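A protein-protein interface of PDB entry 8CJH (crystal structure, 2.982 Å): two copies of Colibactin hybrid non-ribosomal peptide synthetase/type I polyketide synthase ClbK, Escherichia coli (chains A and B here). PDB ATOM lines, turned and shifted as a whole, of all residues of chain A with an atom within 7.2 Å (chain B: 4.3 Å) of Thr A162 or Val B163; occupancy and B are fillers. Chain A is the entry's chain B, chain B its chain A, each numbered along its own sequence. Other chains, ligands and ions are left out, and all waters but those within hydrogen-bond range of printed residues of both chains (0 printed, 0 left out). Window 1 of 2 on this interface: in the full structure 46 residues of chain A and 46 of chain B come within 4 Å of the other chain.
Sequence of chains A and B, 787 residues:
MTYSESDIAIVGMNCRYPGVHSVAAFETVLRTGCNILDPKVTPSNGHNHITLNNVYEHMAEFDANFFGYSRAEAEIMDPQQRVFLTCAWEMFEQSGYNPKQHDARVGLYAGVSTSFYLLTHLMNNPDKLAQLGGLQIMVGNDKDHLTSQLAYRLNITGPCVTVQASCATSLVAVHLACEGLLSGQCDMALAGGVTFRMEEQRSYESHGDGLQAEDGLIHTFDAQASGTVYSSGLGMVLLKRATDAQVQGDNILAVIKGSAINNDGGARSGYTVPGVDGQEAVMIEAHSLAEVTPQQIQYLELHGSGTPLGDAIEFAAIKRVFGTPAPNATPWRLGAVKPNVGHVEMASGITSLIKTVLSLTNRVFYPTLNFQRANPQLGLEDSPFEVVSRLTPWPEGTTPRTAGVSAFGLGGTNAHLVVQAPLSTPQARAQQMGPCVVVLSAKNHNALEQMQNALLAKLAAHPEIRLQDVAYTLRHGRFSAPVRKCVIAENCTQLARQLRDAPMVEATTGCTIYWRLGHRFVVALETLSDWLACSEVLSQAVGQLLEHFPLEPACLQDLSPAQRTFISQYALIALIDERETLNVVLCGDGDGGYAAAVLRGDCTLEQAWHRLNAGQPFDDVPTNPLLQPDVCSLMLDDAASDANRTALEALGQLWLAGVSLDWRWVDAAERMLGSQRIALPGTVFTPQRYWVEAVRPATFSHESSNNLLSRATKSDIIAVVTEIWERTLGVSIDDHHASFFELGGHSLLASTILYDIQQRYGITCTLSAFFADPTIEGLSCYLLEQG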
ATOM      1  N   LEU A 108      14.042   2.007 -27.217  1.00  0.00           N
ATOM      2  CA  LEU A 108      13.672   2.767 -26.041  1.00  0.00           C
ATOM      3  C   LEU A 108      12.711   1.944 -25.204  1.00  0.00           C
ATOM      4  O   LEU A 108      11.597   1.621 -25.633  1.00  0.00           O
ATOM      5  CB  LEU A 108      13.030   4.077 -26.479  1.00  0.00           C
ATOM      6  CG  LEU A 108      14.004   5.096 -27.042  1.00  0.00           C
ATOM      7  CD1 LEU A 108      13.266   6.290 -27.621  1.00  0.00           C
ATOM      8  CD2 LEU A 108      14.967   5.548 -25.965  1.00  0.00           C
ATOM      9  N   TYR A 109      13.180   1.612 -24.008  1.00  0.00           N
ATOM     10  CA  TYR A 109      12.379   0.864 -23.070  1.00  0.00           C
ATOM     11  C   TYR A 109      12.386   1.615 -21.753  1.00  0.00           C
ATOM     12  O   TYR A 109      13.407   1.654 -21.043  1.00  0.00           O
ATOM     13  CB  TYR A 109      12.950  -0.539 -22.934  1.00  0.00           C
ATOM     14  CG  TYR A 109      12.976  -1.333 -24.213  1.00  0.00           C
ATOM     15  CD1 TYR A 109      11.846  -1.993 -24.659  1.00  0.00           C
ATOM     16  CD2 TYR A 109      14.117  -1.406 -24.988  1.00  0.00           C
ATOM     17  CE1 TYR A 109      11.859  -2.740 -25.825  1.00  0.00           C
ATOM     18  CE2 TYR A 109      14.146  -2.141 -26.161  1.00  0.00           C
ATOM     19  CZ  TYR A 109      13.015  -2.813 -26.579  1.00  0.00           C
ATOM     20  OH  TYR A 109      13.047  -3.545 -27.741  1.00  0.00           O
ATOM     21  N   ALA A 110      11.252   2.239 -21.429  1.00  0.00           N
ATOM     22  CA  ALA A 110      11.273   3.062 -20.232  1.00  0.00           C
ATOM     23  C   ALA A 110       9.882   3.333 -19.697  1.00  0.00           C
ATOM     24  O   ALA A 110       8.890   3.242 -20.418  1.00  0.00           O
ATOM     25  CB  ALA A 110      11.988   4.359 -20.527  1.00  0.00           C
ATOM     26  N   GLY A 111       9.856   3.700 -18.415  1.00  0.00           N
ATOM     27  CA  GLY A 111       8.605   3.899 -17.701  1.00  0.00           C
ATOM     28  C   GLY A 111       8.628   5.126 -16.797  1.00  0.00           C
ATOM     29  O   GLY A 111       9.694   5.663 -16.445  1.00  0.00           O
ATOM     30  N   VAL A 112       7.429   5.545 -16.405  1.00  0.00           N
ATOM     31  CA  VAL A 112       7.270   6.814 -15.727  1.00  0.00           C
ATOM     32  C   VAL A 112       6.073   6.745 -14.785  1.00  0.00           C
ATOM     33  O   VAL A 112       5.085   6.077 -15.069  1.00  0.00           O
ATOM     34  CB  VAL A 112       7.113   7.944 -16.758  1.00  0.00           C
ATOM     35  CG1 VAL A 112       5.913   7.695 -17.648  1.00  0.00           C
ATOM     36  CG2 VAL A 112       7.024   9.314 -16.113  1.00  0.00           C
ATOM     37  N   ASP A 142       0.623  11.898 -20.589  1.00  0.00           N
ATOM     38  CA  ASP A 142       0.310  10.486 -20.697  1.00  0.00           C
ATOM     39  C   ASP A 142       1.621   9.694 -20.843  1.00  0.00           C
ATOM     40  O   ASP A 142       2.416   9.925 -21.760  1.00  0.00           O
ATOM     41  CB  ASP A 142      -0.698  10.258 -21.829  1.00  0.00           C
ATOM     42  CG  ASP A 142      -1.504   8.977 -21.689  1.00  0.00           C
ATOM     43  OD1 ASP A 142      -0.905   7.962 -21.325  1.00  0.00           O
ATOM     44  OD2 ASP A 142      -2.721   8.999 -21.954  1.00  0.00           O
ATOM     45  N   LYS A 143       1.825   8.747 -19.919  1.00  0.00           N
ATOM     46  CA  LYS A 143       3.009   7.904 -19.852  1.00  0.00           C
ATOM     47  C   LYS A 143       3.465   7.448 -21.237  1.00  0.00           C
ATOM     48  O   LYS A 143       4.645   7.474 -21.557  1.00  0.00           O
ATOM     49  CB  LYS A 143       2.712   6.646 -19.028  1.00  0.00           C
ATOM     50  CG  LYS A 143       2.139   6.887 -17.640  1.00  0.00           C
ATOM     51  CD  LYS A 143       2.257   5.700 -16.708  1.00  0.00           C
ATOM     52  CE  LYS A 143       1.836   6.059 -15.300  1.00  0.00           C
ATOM     53  NZ  LYS A 143       2.452   5.166 -14.298  1.00  0.00           N
ATOM     54  N   ASP A 144       2.512   6.994 -22.041  1.00  0.00           N
ATOM     55  CA  ASP A 144       2.774   6.549 -23.397  1.00  0.00           C
ATOM     56  C   ASP A 144       3.847   7.398 -24.074  1.00  0.00           C
ATOM     57  O   ASP A 144       4.736   6.861 -24.726  1.00  0.00           O
ATOM     58  CB  ASP A 144       1.494   6.594 -24.223  1.00  0.00           C
ATOM     59  CG  ASP A 144       0.457   5.589 -23.745  1.00  0.00           C
ATOM     60  OD1 ASP A 144       0.277   5.483 -22.520  1.00  0.00           O
ATOM     61  OD2 ASP A 144      -0.160   4.919 -24.599  1.00  0.00           O
ATOM     62  N   HIS A 145       3.772   8.720 -23.924  1.00  0.00           N
ATOM     63  CA  HIS A 145       4.630   9.591 -24.712  1.00  0.00           C
ATOM     64  C   HIS A 145       6.081   9.554 -24.257  1.00  0.00           C
ATOM     65  O   HIS A 145       6.961   9.843 -25.050  1.00  0.00           O
ATOM     66  CB  HIS A 145       4.035  10.994 -24.757  1.00  0.00           C
ATOM     67  CG  HIS A 145       2.740  10.941 -25.461  1.00  0.00           C
ATOM     68  ND1 HIS A 145       2.652  10.426 -26.731  1.00  0.00           N
ATOM     69  CD2 HIS A 145       1.516  11.287 -25.103  1.00  0.00           C
ATOM     70  CE1 HIS A 145       1.397  10.490 -27.131  1.00  0.00           C
ATOM     71  NE2 HIS A 145       0.689  11.008 -26.158  1.00  0.00           N
ATOM     72  N   LEU A 146       6.335   9.171 -23.009  1.00  0.00           N
ATOM     73  CA  LEU A 146       7.686   9.212 -22.486  1.00  0.00           C
ATOM     74  C   LEU A 146       8.672   8.755 -23.545  1.00  0.00           C
ATOM     75  O   LEU A 146       9.601   9.490 -23.869  1.00  0.00           O
ATOM     76  CB  LEU A 146       7.817   8.314 -21.262  1.00  0.00           C
ATOM     77  CG  LEU A 146       9.228   8.246 -20.696  1.00  0.00           C
ATOM     78  CD1 LEU A 146       9.588   9.563 -19.996  1.00  0.00           C
ATOM     79  CD2 LEU A 146       9.374   7.034 -19.777  1.00  0.00           C
ATOM     80  N   THR A 147       8.470   7.540 -24.065  1.00  0.00           N
ATOM     81  CA  THR A 147       9.388   6.998 -25.050  1.00  0.00           C
ATOM     82  C   THR A 147       9.230   7.750 -26.366  1.00  0.00           C
ATOM     83  O   THR A 147      10.215   8.210 -26.921  1.00  0.00           O
ATOM     84  CB  THR A 147       9.230   5.479 -25.195  1.00  0.00           C
ATOM     85  OG1 THR A 147       7.874   5.209 -25.545  1.00  0.00           O
ATOM     86  CG2 THR A 147       9.622   4.726 -23.937  1.00  0.00           C
ATOM     87  N   SER A 148       7.986   7.923 -26.826  1.00  0.00           N
ATOM     88  CA  SER A 148       7.718   8.465 -28.153  1.00  0.00           C
ATOM     89  C   SER A 148       8.406   9.815 -28.351  1.00  0.00           C
ATOM     90  O   SER A 148       8.956  10.075 -29.418  1.00  0.00           O
ATOM     91  CB  SER A 148       6.243   8.602 -28.379  1.00  0.00           C
ATOM     92  OG  SER A 148       5.590   7.369 -28.139  1.00  0.00           O
ATOM     93  N   CYS A 160      10.095   1.092 -29.586  1.00  0.00           N
ATOM     94  CA  CYS A 160       9.880   2.223 -28.719  1.00  0.00           C
ATOM     95  C   CYS A 160       8.675   1.913 -27.846  1.00  0.00           C
ATOM     96  O   CYS A 160       7.547   1.899 -28.335  1.00  0.00           O
ATOM     97  CB  CYS A 160       9.705   3.474 -29.560  1.00  0.00           C
ATOM     98  SG  CYS A 160       9.594   4.986 -28.575  1.00  0.00           S
ATOM     99  N   VAL A 161       8.940   1.636 -26.559  1.00  0.00           N
ATOM    100  CA  VAL A 161       7.920   1.098 -25.672  1.00  0.00           C
ATOM    101  C   VAL A 161       8.021   1.720 -24.287  1.00  0.00           C
ATOM    102  O   VAL A 161       9.044   1.588 -23.583  1.00  0.00           O
ATOM    103  CB  VAL A 161       8.047  -0.425 -25.560  1.00  0.00           C
ATOM    104  CG1 VAL A 161       7.214  -0.973 -24.424  1.00  0.00           C
ATOM    105  CG2 VAL A 161       7.687  -1.103 -26.859  1.00  0.00           C
ATOM    106  N   THR A 162       6.929   2.382 -23.897  1.00  0.00           N
ATOM    107  CA  THR A 162       6.762   2.786 -22.521  1.00  0.00           C
ATOM    108  C   THR A 162       6.301   1.561 -21.744  1.00  0.00           C
ATOM    109  O   THR A 162       5.206   1.066 -21.964  1.00  0.00           O
ATOM    110  CB  THR A 162       5.801   3.964 -22.381  1.00  0.00           C
ATOM    111  OG1 THR A 162       6.325   5.041 -23.149  1.00  0.00           O
ATOM    112  CG2 THR A 162       5.653   4.417 -20.949  1.00  0.00           C
ATOM    113  N   VAL A 163       7.166   1.077 -20.853  1.00  0.00           N
ATOM    114  CA  VAL A 163       6.888  -0.110 -20.066  1.00  0.00           C
ATOM    115  C   VAL A 163       6.521   0.328 -18.654  1.00  0.00           C
ATOM    116  O   VAL A 163       7.116   1.255 -18.127  1.00  0.00           O
ATOM    117  CB  VAL A 163       8.101  -1.059 -20.072  1.00  0.00           C
ATOM    118  CG1 VAL A 163       9.350  -0.407 -19.501  1.00  0.00           C
ATOM    119  CG2 VAL A 163       7.816  -2.349 -19.333  1.00  0.00           C
ATOM    120  N   GLN A 164       5.538  -0.343 -18.047  1.00  0.00           N
ATOM    121  CA  GLN A 164       5.042   0.023 -16.726  1.00  0.00           C
ATOM    122  C   GLN A 164       4.826  -1.231 -15.888  1.00  0.00           C
ATOM    123  O   GLN A 164       4.154  -2.148 -16.333  1.00  0.00           O
ATOM    124  CB  GLN A 164       3.722   0.785 -16.863  1.00  0.00           C
ATOM    125  CG  GLN A 164       3.829   2.126 -17.594  1.00  0.00           C
ATOM    126  CD  GLN A 164       4.753   3.123 -16.935  1.00  0.00           C
ATOM    127  OE1 GLN A 164       5.406   3.929 -17.595  1.00  0.00           O
ATOM    128  NE2 GLN A 164       4.791   3.109 -15.614  1.00  0.00           N
ATOM    129  N   THR A 169       9.367  -1.517 -12.756  1.00  0.00           N
ATOM    130  CA  THR A 169       9.342  -0.904 -14.076  1.00  0.00           C
ATOM    131  C   THR A 169      10.745  -0.811 -14.667  1.00  0.00           C
ATOM    132  O   THR A 169      11.003  -1.459 -15.672  1.00  0.00           O
ATOM    133  CB  THR A 169       8.678   0.472 -14.054  1.00  0.00           C
ATOM    134  OG1 THR A 169       7.371   0.334 -13.501  1.00  0.00           O
ATOM    135  CG2 THR A 169       8.571   1.088 -15.431  1.00  0.00           C
ATOM    136  N   LEU A 176      13.324  -6.120 -21.009  1.00  0.00           N
ATOM    137  CA  LEU A 176      12.740  -6.020 -22.340  1.00  0.00           C
ATOM    138  C   LEU A 176      13.750  -5.461 -23.336  1.00  0.00           C
ATOM    139  O   LEU A 176      13.677  -5.780 -24.517  1.00  0.00           O
ATOM    140  CB  LEU A 176      11.496  -5.136 -22.297  1.00  0.00           C
ATOM    141  CG  LEU A 176      10.283  -5.741 -21.594  1.00  0.00           C
ATOM    142  CD1 LEU A 176       9.068  -4.851 -21.743  1.00  0.00           C
ATOM    143  CD2 LEU A 176       9.965  -7.116 -22.132  1.00  0.00           C
ATOM    144  N   TYR B 109       0.392  -9.094 -21.368  1.00  0.00           N
ATOM    145  CA  TYR B 109       0.883  -7.941 -22.080  1.00  0.00           C
ATOM    146  C   TYR B 109      -0.310  -7.065 -22.425  1.00  0.00           C
ATOM    147  O   TYR B 109      -1.119  -7.411 -23.292  1.00  0.00           O
ATOM    148  CB  TYR B 109       1.660  -8.399 -23.306  1.00  0.00           C
ATOM    149  CG  TYR B 109       2.830  -9.296 -23.001  1.00  0.00           C
ATOM    150  CD1 TYR B 109       2.660 -10.652 -22.786  1.00  0.00           C
ATOM    151  CD2 TYR B 109       4.115  -8.790 -22.938  1.00  0.00           C
ATOM    152  CE1 TYR B 109       3.734 -11.484 -22.524  1.00  0.00           C
ATOM    153  CE2 TYR B 109       5.204  -9.609 -22.682  1.00  0.00           C
ATOM    154  CZ  TYR B 109       5.011 -10.962 -22.467  1.00  0.00           C
ATOM    155  OH  TYR B 109       6.086 -11.768 -22.207  1.00  0.00           O
ATOM    156  N   ALA B 110      -0.442  -5.935 -21.728  1.00  0.00           N
ATOM    157  CA  ALA B 110      -1.627  -5.132 -21.974  1.00  0.00           C
ATOM    158  C   ALA B 110      -1.446  -3.683 -21.545  1.00  0.00           C
ATOM    159  O   ALA B 110      -0.594  -3.357 -20.709  1.00  0.00           O
ATOM    160  CB  ALA B 110      -2.805  -5.752 -21.276  1.00  0.00           C
ATOM    161  N   GLY B 111      -2.297  -2.834 -22.131  1.00  0.00           N
ATOM    162  CA  GLY B 111      -2.206  -1.401 -21.919  1.00  0.00           C
ATOM    163  C   GLY B 111      -3.567  -0.736 -21.754  1.00  0.00           C
ATOM    164  O   GLY B 111      -4.616  -1.295 -22.113  1.00  0.00           O
ATOM    165  N   VAL B 161       3.438  -7.382 -17.870  1.00  0.00           N
ATOM    166  CA  VAL B 161       3.906  -6.089 -18.339  1.00  0.00           C
ATOM    167  C   VAL B 161       2.751  -5.245 -18.859  1.00  0.00           C
ATOM    168  O   VAL B 161       2.062  -5.614 -19.820  1.00  0.00           O
ATOM    169  CB  VAL B 161       4.963  -6.264 -19.435  1.00  0.00           C
ATOM    170  CG1 VAL B 161       5.229  -4.958 -20.164  1.00  0.00           C
ATOM    171  CG2 VAL B 161       6.246  -6.846 -18.870  1.00  0.00           C
ATOM    172  N   THR B 162       2.561  -4.094 -18.212  1.00  0.00           N
ATOM    173  CA  THR B 162       1.696  -3.070 -18.755  1.00  0.00           C
ATOM    174  C   THR B 162       2.490  -2.339 -19.826  1.00  0.00           C
ATOM    175  O   THR B 162       3.477  -1.670 -19.525  1.00  0.00           O
ATOM    176  CB  THR B 162       1.165  -2.126 -17.677  1.00  0.00           C
ATOM    177  OG1 THR B 162       0.438  -2.920 -16.739  1.00  0.00           O
ATOM    178  CG2 THR B 162       0.263  -1.055 -18.248  1.00  0.00           C
ATOM    179  N   VAL B 163       2.050  -2.508 -21.072  1.00  0.00           N
ATOM    180  CA  VAL B 163       2.718  -1.917 -22.213  1.00  0.00           C
ATOM    181  C   VAL B 163       1.910  -0.702 -22.666  1.00  0.00           C
ATOM    182  O   VAL B 163       0.690  -0.742 -22.674  1.00  0.00           O
ATOM    183  CB  VAL B 163       2.884  -2.956 -23.335  1.00  0.00           C
ATOM    184  CG1 VAL B 163       1.568  -3.494 -23.789  1.00  0.00           C
ATOM    185  CG2 VAL B 163       3.619  -2.400 -24.535  1.00  0.00           C
ATOM    186  N   GLN B 164       2.610   0.373 -23.036  1.00  0.00           N
ATOM    187  CA  GLN B 164       1.975   1.618 -23.427  1.00  0.00           C
ATOM    188  C   GLN B 164       2.673   2.181 -24.659  1.00  0.00           C
ATOM    189  O   GLN B 164       3.897   2.295 -24.677  1.00  0.00           O
ATOM    190  CB  GLN B 164       2.045   2.626 -22.285  1.00  0.00           C
ATOM    191  CG  GLN B 164       1.261   2.223 -21.040  1.00  0.00           C
ATOM    192  CD  GLN B 164      -0.217   2.018 -21.260  1.00  0.00           C
ATOM    193  OE1 GLN B 164      -0.836   1.182 -20.611  1.00  0.00           O
ATOM    194  NE2 GLN B 164      -0.814   2.813 -22.132  1.00  0.00           N
ATOM    195  N   THR B 169      -0.654   0.717 -28.767  1.00  0.00           N
ATOM    196  CA  THR B 169      -0.506  -0.036 -27.529  1.00  0.00           C
ATOM    197  C   THR B 169      -0.893  -1.501 -27.714  1.00  0.00           C
ATOM    198  O   THR B 169      -0.040  -2.379 -27.601  1.00  0.00           O
ATOM    199  CB  THR B 169      -1.285   0.607 -26.379  1.00  0.00           C
ATOM    200  OG1 THR B 169      -0.814   1.945 -26.224  1.00  0.00           O
ATOM    201  CG2 THR B 169      -1.102  -0.121 -25.072  1.00  0.00           C
ATOM    202  N   VAL B 172       1.357  -3.411 -29.977  1.00  0.00           N
ATOM    203  CA  VAL B 172       2.680  -3.507 -29.394  1.00  0.00           C
ATOM    204  C   VAL B 172       2.658  -4.643 -28.364  1.00  0.00           C
ATOM    205  O   VAL B 172       3.549  -5.501 -28.336  1.00  0.00           O
ATOM    206  CB  VAL B 172       3.111  -2.157 -28.804  1.00  0.00           C
ATOM    207  CG1 VAL B 172       4.430  -2.256 -28.057  1.00  0.00           C
ATOM    208  CG2 VAL B 172       3.192  -1.098 -29.892  1.00  0.00           C
ATOM    209  N   ALA B 173       1.605  -4.645 -27.541  1.00  0.00           N
ATOM    210  CA  ALA B 173       1.343  -5.725 -26.603  1.00  0.00           C
ATOM    211  C   ALA B 173       1.370  -7.077 -27.301  1.00  0.00           C
ATOM    212  O   ALA B 173       2.097  -7.982 -26.886  1.00  0.00           O
ATOM    213  CB  ALA B 173       0.000  -5.532 -25.937  1.00  0.00           C
ATOM    214  N   LEU B 176       4.953  -7.924 -28.187  1.00  0.00           N
ATOM    215  CA  LEU B 176       5.742  -8.299 -27.025  1.00  0.00           C
ATOM    216  C   LEU B 176       5.313  -9.655 -26.482  1.00  0.00           C
ATOM    217  O   LEU B 176       6.132 -10.357 -25.895  1.00  0.00           O
ATOM    218  CB  LEU B 176       5.605  -7.214 -25.958  1.00  0.00           C
ATOM    219  CG  LEU B 176       6.358  -5.927 -26.287  1.00  0.00           C
ATOM    220  CD1 LEU B 176       6.227  -4.923 -25.161  1.00  0.00           C
ATOM    221  CD2 LEU B 176       7.832  -6.225 -26.570  1.00  0.00           C
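Val A161 touches Val B163, and with the chains exchanged Val A163 touches Val B161.
Thr A162 touches Val B163, and with the chains exchanged Val A163 touches Thr B162.
Thr A162 touches Gln B164, and with the chains exchanged Gln A164 touches Thr B162.
Of the 9 pairs that touch across the chains among the printed residues, 6 have their exchanged pair printed and touching as well.
Val B163 touches Val A161 (CG2 to CG1, 3.9 Å).
Val A161 touches Val B172.
O of Thr A162 touches C of Val B163, 3.8 Å away.
Val A163 touches Val B161.
Val A163 touches Thr B162.
The backbone carbonyl oxygen (O) of Thr B162 sits at hydrogen-bond distance from the backbone NH (N) of Gln A164 (2.9 Å).
OD1 of Asp A144 sits at hydrogen-bond distance from NE2 of Gln B164 (2.9 Å).
N of Gln B164 is in hydrogen-bond range of O of Thr A162 (2.9 Å).
The side-chain hydroxyl (OG1) of Thr B169 lies within hydrogen-bond range of the side-chain carboxylate (OD2) of Asp A144 (3.5 Å).
Along chain A the printed residues that touch a printed residue of chain B span positions 144 to 164.
Of the 11 printed residues of chain B, 6 touch a printed residue of chain A.
Hydrophobic or aromatic side chains of chain B that line the printed part of chain A: Val B161, Val B163 and Val B172.
Among the printed residues, 9 pairs touch across the chains.
Among the printed residues, no Asp or Glu carboxylate lies within 4 Å of a Lys or Arg side-chain nitrogen of the other chain.
Val A112 touches none of the printed residues of chain B.
Thr A162 touches just these residues of chain B: Val B163 (3.8 Å) and Gln B164 (2.9 Å).
Of chain A, only Val A161 (3.9 Å) and Thr A162 (3.8 Å) come within 4 Å of Val B163.
Of the printed residues of chain A, Gln B164 touches Asp A144 (2.9 Å) and Thr A162 (2.9 Å).
Of the printed residues of chain A, Thr B169 touches Asp A144 (3.5 Å).
The nearest residue of chain A that does not touch Val B163 is Val A163 (5.0 Å).
The nearest printed residue of chain B that does not touch Gln A164 is Val B161 (4.2 Å).
The backbone carbonyl oxygen of Ala B110 lies within hydrogen-bond range of the backbone NH of Val B163.
The backbone NH (N) of Val A161 lies within hydrogen-bond range of the backbone carbonyl oxygen (O) of Leu A108 (2.8 Å).
The backbone NH of Ala A110 sits at hydrogen-bond distance from the backbone carbonyl oxygen of Val A161, at 3.2 Å.
The side-chain amide nitrogen (NE2) of Gln A164 lies close to the side-chain amino group (NZ) of Lys A143 (3.4 Å).
The backbone carbonyl oxygen (O) of Asp A144 sits at hydrogen-bond distance from the side-chain hydroxyl (OG1) of Thr A162.
The side-chain hydroxyl (OG1) of Thr A147 is in hydrogen-bond range of the side-chain hydroxyl (OG1) of Thr A162 (2.9 Å).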
